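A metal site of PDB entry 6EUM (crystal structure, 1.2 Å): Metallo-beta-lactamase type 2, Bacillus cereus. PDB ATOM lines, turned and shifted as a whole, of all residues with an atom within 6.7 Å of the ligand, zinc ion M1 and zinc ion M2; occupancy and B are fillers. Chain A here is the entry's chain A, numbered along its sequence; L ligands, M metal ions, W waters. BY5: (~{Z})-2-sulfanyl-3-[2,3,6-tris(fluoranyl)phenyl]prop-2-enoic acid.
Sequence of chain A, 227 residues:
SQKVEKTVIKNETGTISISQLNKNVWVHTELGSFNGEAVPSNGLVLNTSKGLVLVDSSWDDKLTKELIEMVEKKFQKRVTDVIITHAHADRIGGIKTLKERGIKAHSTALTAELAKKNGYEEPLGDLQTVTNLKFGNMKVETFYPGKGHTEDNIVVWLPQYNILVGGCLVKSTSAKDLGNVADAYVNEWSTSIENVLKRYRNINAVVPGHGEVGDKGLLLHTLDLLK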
ATOM      1  N   PHE A  34     -20.953  34.955  20.133  1.00  0.00           N
ATOM      2  CA  PHE A  34     -20.153  35.163  18.931  1.00  0.00           C
ATOM      3  C   PHE A  34     -21.065  35.636  17.804  1.00  0.00           C
ATOM      4  O   PHE A  34     -21.784  34.834  17.182  1.00  0.00           O
ATOM      5  CB  PHE A  34     -19.413  33.883  18.564  1.00  0.00           C
ATOM      6  CG  PHE A  34     -18.453  33.452  19.631  1.00  0.00           C
ATOM      7  CD1 PHE A  34     -17.150  33.914  19.635  1.00  0.00           C
ATOM      8  CD2 PHE A  34     -18.870  32.613  20.644  1.00  0.00           C
ATOM      9  CE1 PHE A  34     -16.262  33.533  20.611  1.00  0.00           C
ATOM     10  CE2 PHE A  34     -18.000  32.224  21.619  1.00  0.00           C
ATOM     11  CZ  PHE A  34     -16.687  32.687  21.614  1.00  0.00           C
ATOM     12  N   VAL A  39     -22.990  30.266  22.173  1.00  0.00           N
ATOM     13  CA  VAL A  39     -22.396  28.970  21.885  1.00  0.00           C
ATOM     14  C   VAL A  39     -21.962  28.389  23.230  1.00  0.00           C
ATOM     15  O   VAL A  39     -21.004  28.874  23.855  1.00  0.00           O
ATOM     16  CB  VAL A  39     -21.173  29.111  20.983  1.00  0.00           C
ATOM     17  CG1 VAL A  39     -20.637  27.772  20.646  1.00  0.00           C
ATOM     18  CG2 VAL A  39     -21.553  29.925  19.707  1.00  0.00           C
ATOM     19  N   SER A  41     -20.298  25.767  25.972  1.00  0.00           N
ATOM     20  CA  SER A  41     -19.228  24.797  26.053  1.00  0.00           C
ATOM     21  C   SER A  41     -19.119  24.239  27.469  1.00  0.00           C
ATOM     22  O   SER A  41     -19.364  24.951  28.452  1.00  0.00           O
ATOM     23  CB  SER A  41     -17.892  25.404  25.632  1.00  0.00           C
ATOM     24  OG  SER A  41     -17.526  26.366  26.561  1.00  0.00           O
ATOM     25  N   TRP A  59     -14.242  30.321  27.586  1.00  0.00           N
ATOM     26  CA  TRP A  59     -13.941  31.085  26.356  1.00  0.00           C
ATOM     27  C   TRP A  59     -13.028  32.245  26.580  1.00  0.00           C
ATOM     28  O   TRP A  59     -12.354  32.668  25.617  1.00  0.00           O
ATOM     29  CB  TRP A  59     -15.275  31.638  25.809  1.00  0.00           C
ATOM     30  CG  TRP A  59     -16.255  30.598  25.375  1.00  0.00           C
ATOM     31  CD1 TRP A  59     -17.371  30.125  26.084  1.00  0.00           C
ATOM     32  CD2 TRP A  59     -16.283  29.929  24.113  1.00  0.00           C
ATOM     33  NE1 TRP A  59     -18.051  29.236  25.317  1.00  0.00           N
ATOM     34  CE2 TRP A  59     -17.395  29.059  24.103  1.00  0.00           C
ATOM     35  CE3 TRP A  59     -15.450  29.974  22.990  1.00  0.00           C
ATOM     36  CZ2 TRP A  59     -17.732  28.294  22.974  1.00  0.00           C
ATOM     37  CZ3 TRP A  59     -15.810  29.214  21.867  1.00  0.00           C
ATOM     38  CH2 TRP A  59     -16.901  28.344  21.892  1.00  0.00           C
ATOM     39  N   HIS A  86      -7.331  20.952  24.820  1.00  0.00           N
ATOM     40  CA  HIS A  86      -6.714  21.342  23.540  1.00  0.00           C
ATOM     41  C   HIS A  86      -6.557  22.848  23.555  1.00  0.00           C
ATOM     42  O   HIS A  86      -7.002  23.524  24.476  1.00  0.00           O
ATOM     43  CB  HIS A  86      -7.391  20.833  22.274  1.00  0.00           C
ATOM     44  CG  HIS A  86      -8.742  21.341  21.952  1.00  0.00           C
ATOM     45  ND1 HIS A  86      -9.889  20.872  22.528  1.00  0.00           N
ATOM     46  CD2 HIS A  86      -9.151  22.211  20.994  1.00  0.00           C
ATOM     47  CE1 HIS A  86     -10.933  21.482  21.974  1.00  0.00           C
ATOM     48  NE2 HIS A  86     -10.521  22.304  21.040  1.00  0.00           N
ATOM     49  N   ALA A  87      -5.903  23.377  22.532  1.00  0.00           N
ATOM     50  CA  ALA A  87      -5.505  24.800  22.495  1.00  0.00           C
ATOM     51  C   ALA A  87      -6.466  25.693  21.700  1.00  0.00           C
ATOM     52  O   ALA A  87      -6.035  26.862  21.421  1.00  0.00           O
ATOM     53  CB  ALA A  87      -4.094  24.943  21.929  1.00  0.00           C
ATOM     54  N   HIS A  88      -7.750  25.473  21.735  1.00  0.00           N
ATOM     55  CA  HIS A  88      -8.770  26.417  21.245  1.00  0.00           C
ATOM     56  C   HIS A  88      -9.336  27.269  22.419  1.00  0.00           C
ATOM     57  O   HIS A  88      -9.335  26.853  23.579  1.00  0.00           O
ATOM     58  CB  HIS A  88      -9.928  25.685  20.554  1.00  0.00           C
ATOM     59  CG  HIS A  88      -9.608  25.174  19.186  1.00  0.00           C
ATOM     60  ND1 HIS A  88     -10.398  24.177  18.607  1.00  0.00           N
ATOM     61  CD2 HIS A  88      -8.721  25.582  18.229  1.00  0.00           C
ATOM     62  CE1 HIS A  88      -9.984  24.063  17.367  1.00  0.00           C
ATOM     63  NE2 HIS A  88      -8.976  24.854  17.111  1.00  0.00           N
ATOM     64  N   ALA A  89      -9.979  28.394  22.086  1.00  0.00           N
ATOM     65  CA  ALA A  89     -10.414  29.383  23.065  1.00  0.00           C
ATOM     66  C   ALA A  89     -11.405  28.807  24.083  1.00  0.00           C
ATOM     67  O   ALA A  89     -11.371  29.229  25.237  1.00  0.00           O
ATOM     68  CB  ALA A  89     -11.041  30.589  22.367  1.00  0.00           C
ATOM     69  N   ASP A  90     -12.316  27.910  23.677  1.00  0.00           N
ATOM     70  CA  ASP A  90     -13.274  27.363  24.648  1.00  0.00           C
ATOM     71  C   ASP A  90     -12.570  26.633  25.775  1.00  0.00           C
ATOM     72  O   ASP A  90     -13.111  26.588  26.888  1.00  0.00           O
ATOM     73  CB  ASP A  90     -14.346  26.475  23.936  1.00  0.00           C
ATOM     74  CG  ASP A  90     -13.843  25.260  23.192  1.00  0.00           C
ATOM     75  OD1 ASP A  90     -12.679  25.318  22.691  1.00  0.00           O
ATOM     76  OD2 ASP A  90     -14.578  24.215  23.074  1.00  0.00           O
ATOM     77  N   ARG A  91     -11.437  25.995  25.521  1.00  0.00           N
ATOM     78  CA  ARG A  91     -10.691  25.223  26.498  1.00  0.00           C
ATOM     79  C   ARG A  91      -9.726  26.076  27.290  1.00  0.00           C
ATOM     80  O   ARG A  91      -9.589  25.933  28.508  1.00  0.00           O
ATOM     81  CB  ARG A  91      -9.898  24.170  25.777  1.00  0.00           C
ATOM     82  CG  ARG A  91     -10.667  23.266  24.830  1.00  0.00           C
ATOM     83  CD  ARG A  91     -11.677  22.332  25.453  1.00  0.00           C
ATOM     84  NE  ARG A  91     -13.041  22.816  25.232  1.00  0.00           N
ATOM     85  CZ  ARG A  91     -14.097  22.436  25.909  1.00  0.00           C
ATOM     86  NH1 ARG A  91     -13.962  21.598  26.910  1.00  0.00           N
ATOM     87  NH2 ARG A  91     -15.262  22.810  25.522  1.00  0.00           N
ATOM     88  N   TYR A 120      -1.474  32.518  23.174  1.00  0.00           N
ATOM     89  CA  TYR A 120      -1.903  32.321  24.547  1.00  0.00           C
ATOM     90  C   TYR A 120      -0.730  32.063  25.483  1.00  0.00           C
ATOM     91  O   TYR A 120       0.311  31.522  25.077  1.00  0.00           O
ATOM     92  CB  TYR A 120      -2.833  31.087  24.590  1.00  0.00           C
ATOM     93  CG  TYR A 120      -4.208  31.296  24.001  1.00  0.00           C
ATOM     94  CD1 TYR A 120      -5.098  32.172  24.575  1.00  0.00           C
ATOM     95  CD2 TYR A 120      -4.629  30.552  22.894  1.00  0.00           C
ATOM     96  CE1 TYR A 120      -6.343  32.378  24.049  1.00  0.00           C
ATOM     97  CE2 TYR A 120      -5.897  30.737  22.309  1.00  0.00           C
ATOM     98  CZ  TYR A 120      -6.756  31.669  22.879  1.00  0.00           C
ATOM     99  OH  TYR A 120      -8.006  31.835  22.313  1.00  0.00           O
ATOM    100  N   HIS A 149     -10.500  16.232  16.306  1.00  0.00           N
ATOM    101  CA  HIS A 149     -10.965  17.599  16.229  1.00  0.00           C
ATOM    102  C   HIS A 149      -9.822  18.610  16.101  1.00  0.00           C
ATOM    103  O   HIS A 149      -9.927  19.549  15.327  1.00  0.00           O
ATOM    104  CB  HIS A 149     -11.811  17.893  17.471  1.00  0.00           C
ATOM    105  CG  HIS A 149     -12.070  19.324  17.724  1.00  0.00           C
ATOM    106  ND1 HIS A 149     -12.907  20.071  16.954  1.00  0.00           N
ATOM    107  CD2 HIS A 149     -11.528  20.177  18.631  1.00  0.00           C
ATOM    108  CE1 HIS A 149     -12.921  21.321  17.400  1.00  0.00           C
ATOM    109  NE2 HIS A 149     -12.064  21.458  18.412  1.00  0.00           N
ATOM    110  N   THR A 150      -8.719  18.319  16.793  1.00  0.00           N
ATOM    111  CA  THR A 150      -7.469  19.021  16.614  1.00  0.00           C
ATOM    112  C   THR A 150      -6.361  18.012  16.703  1.00  0.00           C
ATOM    113  O   THR A 150      -6.555  16.844  17.028  1.00  0.00           O
ATOM    114  CB  THR A 150      -7.203  20.090  17.684  1.00  0.00           C
ATOM    115  OG1 THR A 150      -7.235  19.462  18.952  1.00  0.00           O
ATOM    116  CG2 THR A 150      -8.174  21.214  17.599  1.00  0.00           C
ATOM    117  N   GLY A 167     -14.499  15.901  25.544  1.00  0.00           N
ATOM    118  CA  GLY A 167     -14.095  17.171  25.025  1.00  0.00           C
ATOM    119  C   GLY A 167     -14.550  17.258  23.585  1.00  0.00           C
ATOM    120  O   GLY A 167     -15.506  16.631  23.124  1.00  0.00           O
ATOM    121  N   CSO A 168     -13.840  18.060  22.789  1.00  0.00           N
ATOM    122  CA  CSO A 168     -14.364  18.414  21.485  1.00  0.00           C
ATOM    123  CB  CSO A 168     -13.985  19.815  21.121  1.00  0.00           C
ATOM    124  SG  CSO A 168     -14.299  20.991  22.535  1.00  0.00           S
ATOM    125  C   CSO A 168     -14.078  17.343  20.425  1.00  0.00           C
ATOM    126  O   CSO A 168     -14.627  17.432  19.321  1.00  0.00           O
ATOM    127  N   LEU A 169     -13.337  16.318  20.793  1.00  0.00           N
ATOM    128  CA  LEU A 169     -13.247  15.083  20.013  1.00  0.00           C
ATOM    129  C   LEU A 169     -14.587  14.405  19.851  1.00  0.00           C
ATOM    130  O   LEU A 169     -14.792  13.629  18.906  1.00  0.00           O
ATOM    131  CB  LEU A 169     -12.238  14.131  20.728  1.00  0.00           C
ATOM    132  CG  LEU A 169     -11.927  12.829  20.047  1.00  0.00           C
ATOM    133  CD1 LEU A 169     -11.009  13.037  18.842  1.00  0.00           C
ATOM    134  CD2 LEU A 169     -11.280  11.874  21.070  1.00  0.00           C
ATOM    135  N   LYS A 171     -18.722  14.578  19.596  1.00  0.00           N
ATOM    136  CA  LYS A 171     -19.888  15.369  19.304  1.00  0.00           C
ATOM    137  C   LYS A 171     -21.106  14.908  20.090  1.00  0.00           C
ATOM    138  O   LYS A 171     -21.340  13.709  20.291  1.00  0.00           O
ATOM    139  CB  LYS A 171     -20.200  15.321  17.813  1.00  0.00           C
ATOM    140  CG  LYS A 171     -18.992  15.682  16.900  1.00  0.00           C
ATOM    141  CD  LYS A 171     -18.352  16.979  17.111  1.00  0.00           C
ATOM    142  CE  LYS A 171     -19.121  18.121  16.806  1.00  0.00           C
ATOM    143  NZ  LYS A 171     -18.295  19.417  16.940  1.00  0.00           N
ATOM    144  N   LEU A 178     -19.610  18.013  11.785  1.00  0.00           N
ATOM    145  CA  LEU A 178     -18.405  18.024  12.583  1.00  0.00           C
ATOM    146  C   LEU A 178     -18.027  19.393  13.103  1.00  0.00           C
ATOM    147  O   LEU A 178     -17.081  19.480  13.922  1.00  0.00           O
ATOM    148  CB  LEU A 178     -17.255  17.447  11.769  1.00  0.00           C
ATOM    149  CG  LEU A 178     -17.453  15.975  11.417  1.00  0.00           C
ATOM    150  CD1 LEU A 178     -16.374  15.632  10.366  1.00  0.00           C
ATOM    151  CD2 LEU A 178     -17.333  15.135  12.662  1.00  0.00           C
ATOM    152  N   GLY A 179     -18.711  20.440  12.673  1.00  0.00           N
ATOM    153  CA  GLY A 179     -18.381  21.772  13.091  1.00  0.00           C
ATOM    154  C   GLY A 179     -17.130  22.308  12.402  1.00  0.00           C
ATOM    155  O   GLY A 179     -16.857  22.009  11.245  1.00  0.00           O
ATOM    156  N   ASN A 180     -16.360  23.115  13.105  1.00  0.00           N
ATOM    157  CA  ASN A 180     -15.213  23.741  12.488  1.00  0.00           C
ATOM    158  C   ASN A 180     -14.094  22.713  12.372  1.00  0.00           C
ATOM    159  O   ASN A 180     -13.570  22.217  13.373  1.00  0.00           O
ATOM    160  CB  ASN A 180     -14.792  24.942  13.325  1.00  0.00           C
ATOM    161  CG  ASN A 180     -13.742  25.782  12.654  1.00  0.00           C
ATOM    162  OD1 ASN A 180     -12.823  25.253  12.141  1.00  0.00           O
ATOM    163  ND2 ASN A 180     -13.875  27.098  12.688  1.00  0.00           N
ATOM    164  N   VAL A 181     -13.725  22.421  11.131  1.00  0.00           N
ATOM    165  CA  VAL A 181     -12.721  21.416  10.841  1.00  0.00           C
ATOM    166  C   VAL A 181     -11.448  22.050  10.262  1.00  0.00           C
ATOM    167  O   VAL A 181     -10.528  21.307   9.819  1.00  0.00           O
ATOM    168  CB  VAL A 181     -13.270  20.317   9.929  1.00  0.00           C
ATOM    169  CG1 VAL A 181     -14.351  19.527  10.642  1.00  0.00           C
ATOM    170  CG2 VAL A 181     -13.846  20.953   8.607  1.00  0.00           C
ATOM    171  N   ALA A 182     -11.257  23.336  10.472  1.00  0.00           N
ATOM    172  CA  ALA A 182     -10.032  23.953   9.987  1.00  0.00           C
ATOM    173  C   ALA A 182      -8.791  23.333  10.574  1.00  0.00           C
ATOM    174  O   ALA A 182      -7.776  23.182   9.875  1.00  0.00           O
ATOM    175  CB  ALA A 182     -10.025  25.443  10.292  1.00  0.00           C
ATOM    176  N   ASP A 183      -8.816  22.950  11.847  1.00  0.00           N
ATOM    177  CA  ASP A 183      -7.698  22.388  12.535  1.00  0.00           C
ATOM    178  C   ASP A 183      -7.833  20.898  12.742  1.00  0.00           C
ATOM    179  O   ASP A 183      -7.019  20.312  13.476  1.00  0.00           O
ATOM    180  CB  ASP A 183      -7.534  23.089  13.882  1.00  0.00           C
ATOM    181  CG  ASP A 183      -7.250  24.581  13.761  1.00  0.00           C
ATOM    182  OD1 ASP A 183      -6.580  24.990  12.824  1.00  0.00           O
ATOM    183  OD2 ASP A 183      -7.681  25.328  14.672  1.00  0.00           O
ATOM    184  N   GLY A 209     -17.613  18.120  24.383  1.00  0.00           N
ATOM    185  CA  GLY A 209     -17.164  19.491  24.541  1.00  0.00           C
ATOM    186  C   GLY A 209     -18.293  20.523  24.505  1.00  0.00           C
ATOM    187  O   GLY A 209     -18.203  21.591  25.112  1.00  0.00           O
ATOM    188  N   HIS A 210     -19.336  20.224  23.741  1.00  0.00           N
ATOM    189  CA  HIS A 210     -20.493  21.069  23.550  1.00  0.00           C
ATOM    190  C   HIS A 210     -21.715  20.148  23.551  1.00  0.00           C
ATOM    191  O   HIS A 210     -21.705  19.129  22.878  1.00  0.00           O
ATOM    192  CB  HIS A 210     -20.387  21.889  22.198  1.00  0.00           C
ATOM    193  CG  HIS A 210     -19.051  22.614  22.077  1.00  0.00           C
ATOM    194  ND1 HIS A 210     -18.799  23.870  22.584  1.00  0.00           N
ATOM    195  CD2 HIS A 210     -17.860  22.213  21.552  1.00  0.00           C
ATOM    196  CE1 HIS A 210     -17.528  24.181  22.356  1.00  0.00           C
ATOM    197  NE2 HIS A 210     -16.929  23.201  21.729  1.00  0.00           N
HETATM  198  C4  BY5 L   1     -12.559  26.058  16.598  1.00  0.00           C
HETATM  199  C5  BY5 L   1     -11.639  27.083  16.560  1.00  0.00           C
HETATM  200  C6  BY5 L   1     -11.719  28.075  17.528  1.00  0.00           C
HETATM  201  C7  BY5 L   1     -12.730  28.022  18.466  1.00  0.00           C
HETATM  202  C8  BY5 L   1     -13.652  27.006  18.469  1.00  0.00           C
HETATM  203  C   BY5 L   1     -15.531  22.803  18.488  1.00  0.00           C
HETATM  204  O   BY5 L   1     -15.498  22.002  19.483  1.00  0.00           O
HETATM  205  C1  BY5 L   1     -14.620  23.972  18.592  1.00  0.00           C
HETATM  206  C2  BY5 L   1     -14.504  24.809  17.534  1.00  0.00           C
HETATM  207  C3  BY5 L   1     -13.598  25.970  17.533  1.00  0.00           C
HETATM  208  F   BY5 L   1     -12.454  25.054  15.691  1.00  0.00           F
HETATM  209  F1  BY5 L   1     -14.677  27.068  19.335  1.00  0.00           F
HETATM  210  F2  BY5 L   1     -12.833  28.994  19.405  1.00  0.00           F
HETATM  211  O1  BY5 L   1     -16.168  22.551  17.484  1.00  0.00           O
HETATM  212  S   BY5 L   1     -13.642  24.216  20.098  1.00  0.00           S
HETATM  213 ZN    ZN M   1     -14.907  22.926  21.513  1.00  0.00          ZN
HETATM  214 ZN    ZN M   2     -11.682  23.054  19.560  1.00  0.00          ZN
HETATM  215  O   HOH W   1     -17.249  23.938  15.527  1.00  0.00           O
HETATM  216  O   HOH W   2     -16.633  19.470  19.126  1.00  0.00           O
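O1 of the ligand is in salt-bridge range of NZ of Lys 171, 3.8 Å away.
A ring nitrogen (NE2) of His 88 is in hydrogen-bond range of the side-chain carboxylate (OD2) of Asp 183, at 2.8 Å. The side-chain carboxylate of Asp 90 lies within salt-bridge range of the guanidinium group of Arg 91 (3.6 Å). SG of CSO 168 lies close to the guanidinium group (NE) of Arg 91 (3.5 Å). The backbone NH of Ala 182 is in hydrogen-bond range of the side-chain amide oxygen of Asn 180 (3.0 Å). The indole nitrogen of Trp 59 lies within hydrogen-bond range of the side-chain hydroxyl of Ser 41 (3.2 Å). The indole nitrogen (NE1) of Trp 59 sits at hydrogen-bond distance from the backbone carbonyl oxygen (O) of Val 39 (3.3 Å). The side-chain amino group (NZ) of Lys 171 lies within hydrogen-bond range of the backbone carbonyl oxygen (O) of Leu 178 (3.3 Å).
Residues that only touch the ligand: Asn 180 (3.3 Å), Trp 59 (3.5 Å) and Ala 89 (3.8 Å).
Within 4 Å of zinc ion M1: Asp 90, CSO 168 and His 210. The nearest printed residue that does not touch zinc ion M1 is Arg 91 (4.03 Å).
Of the 25 residues printed, 4 come within 4 Å of zinc ion M2.
OD2 of Asp 90 is bound to zinc ion M1 (2.1 Å). A ring nitrogen (NE2) of His 210 is bound to zinc ion M1, at 2.1 Å. SG of CSO 168 binds zinc ion M1. A sulfur (S) of the ligand binds zinc ion M1. O of the ligand is bound to zinc ion M1 (2.3 Å).
Zinc ion M2 is bound by a ring nitrogen (ND1) of His 88 (2.0 Å), a ring nitrogen (NE2) of His 149 (2.0 Å), a ring nitrogen (NE2) of His 86 (2.0 Å) and a sulfur (S) of the ligand (2.3 Å).
Water W1 bridges an oxygen (O1) of the ligand and the backbone NH (N) of Asn 180. Water W2 lies within hydrogen-bond range of the side-chain amino group of Lys 171 and O of CSO 168.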
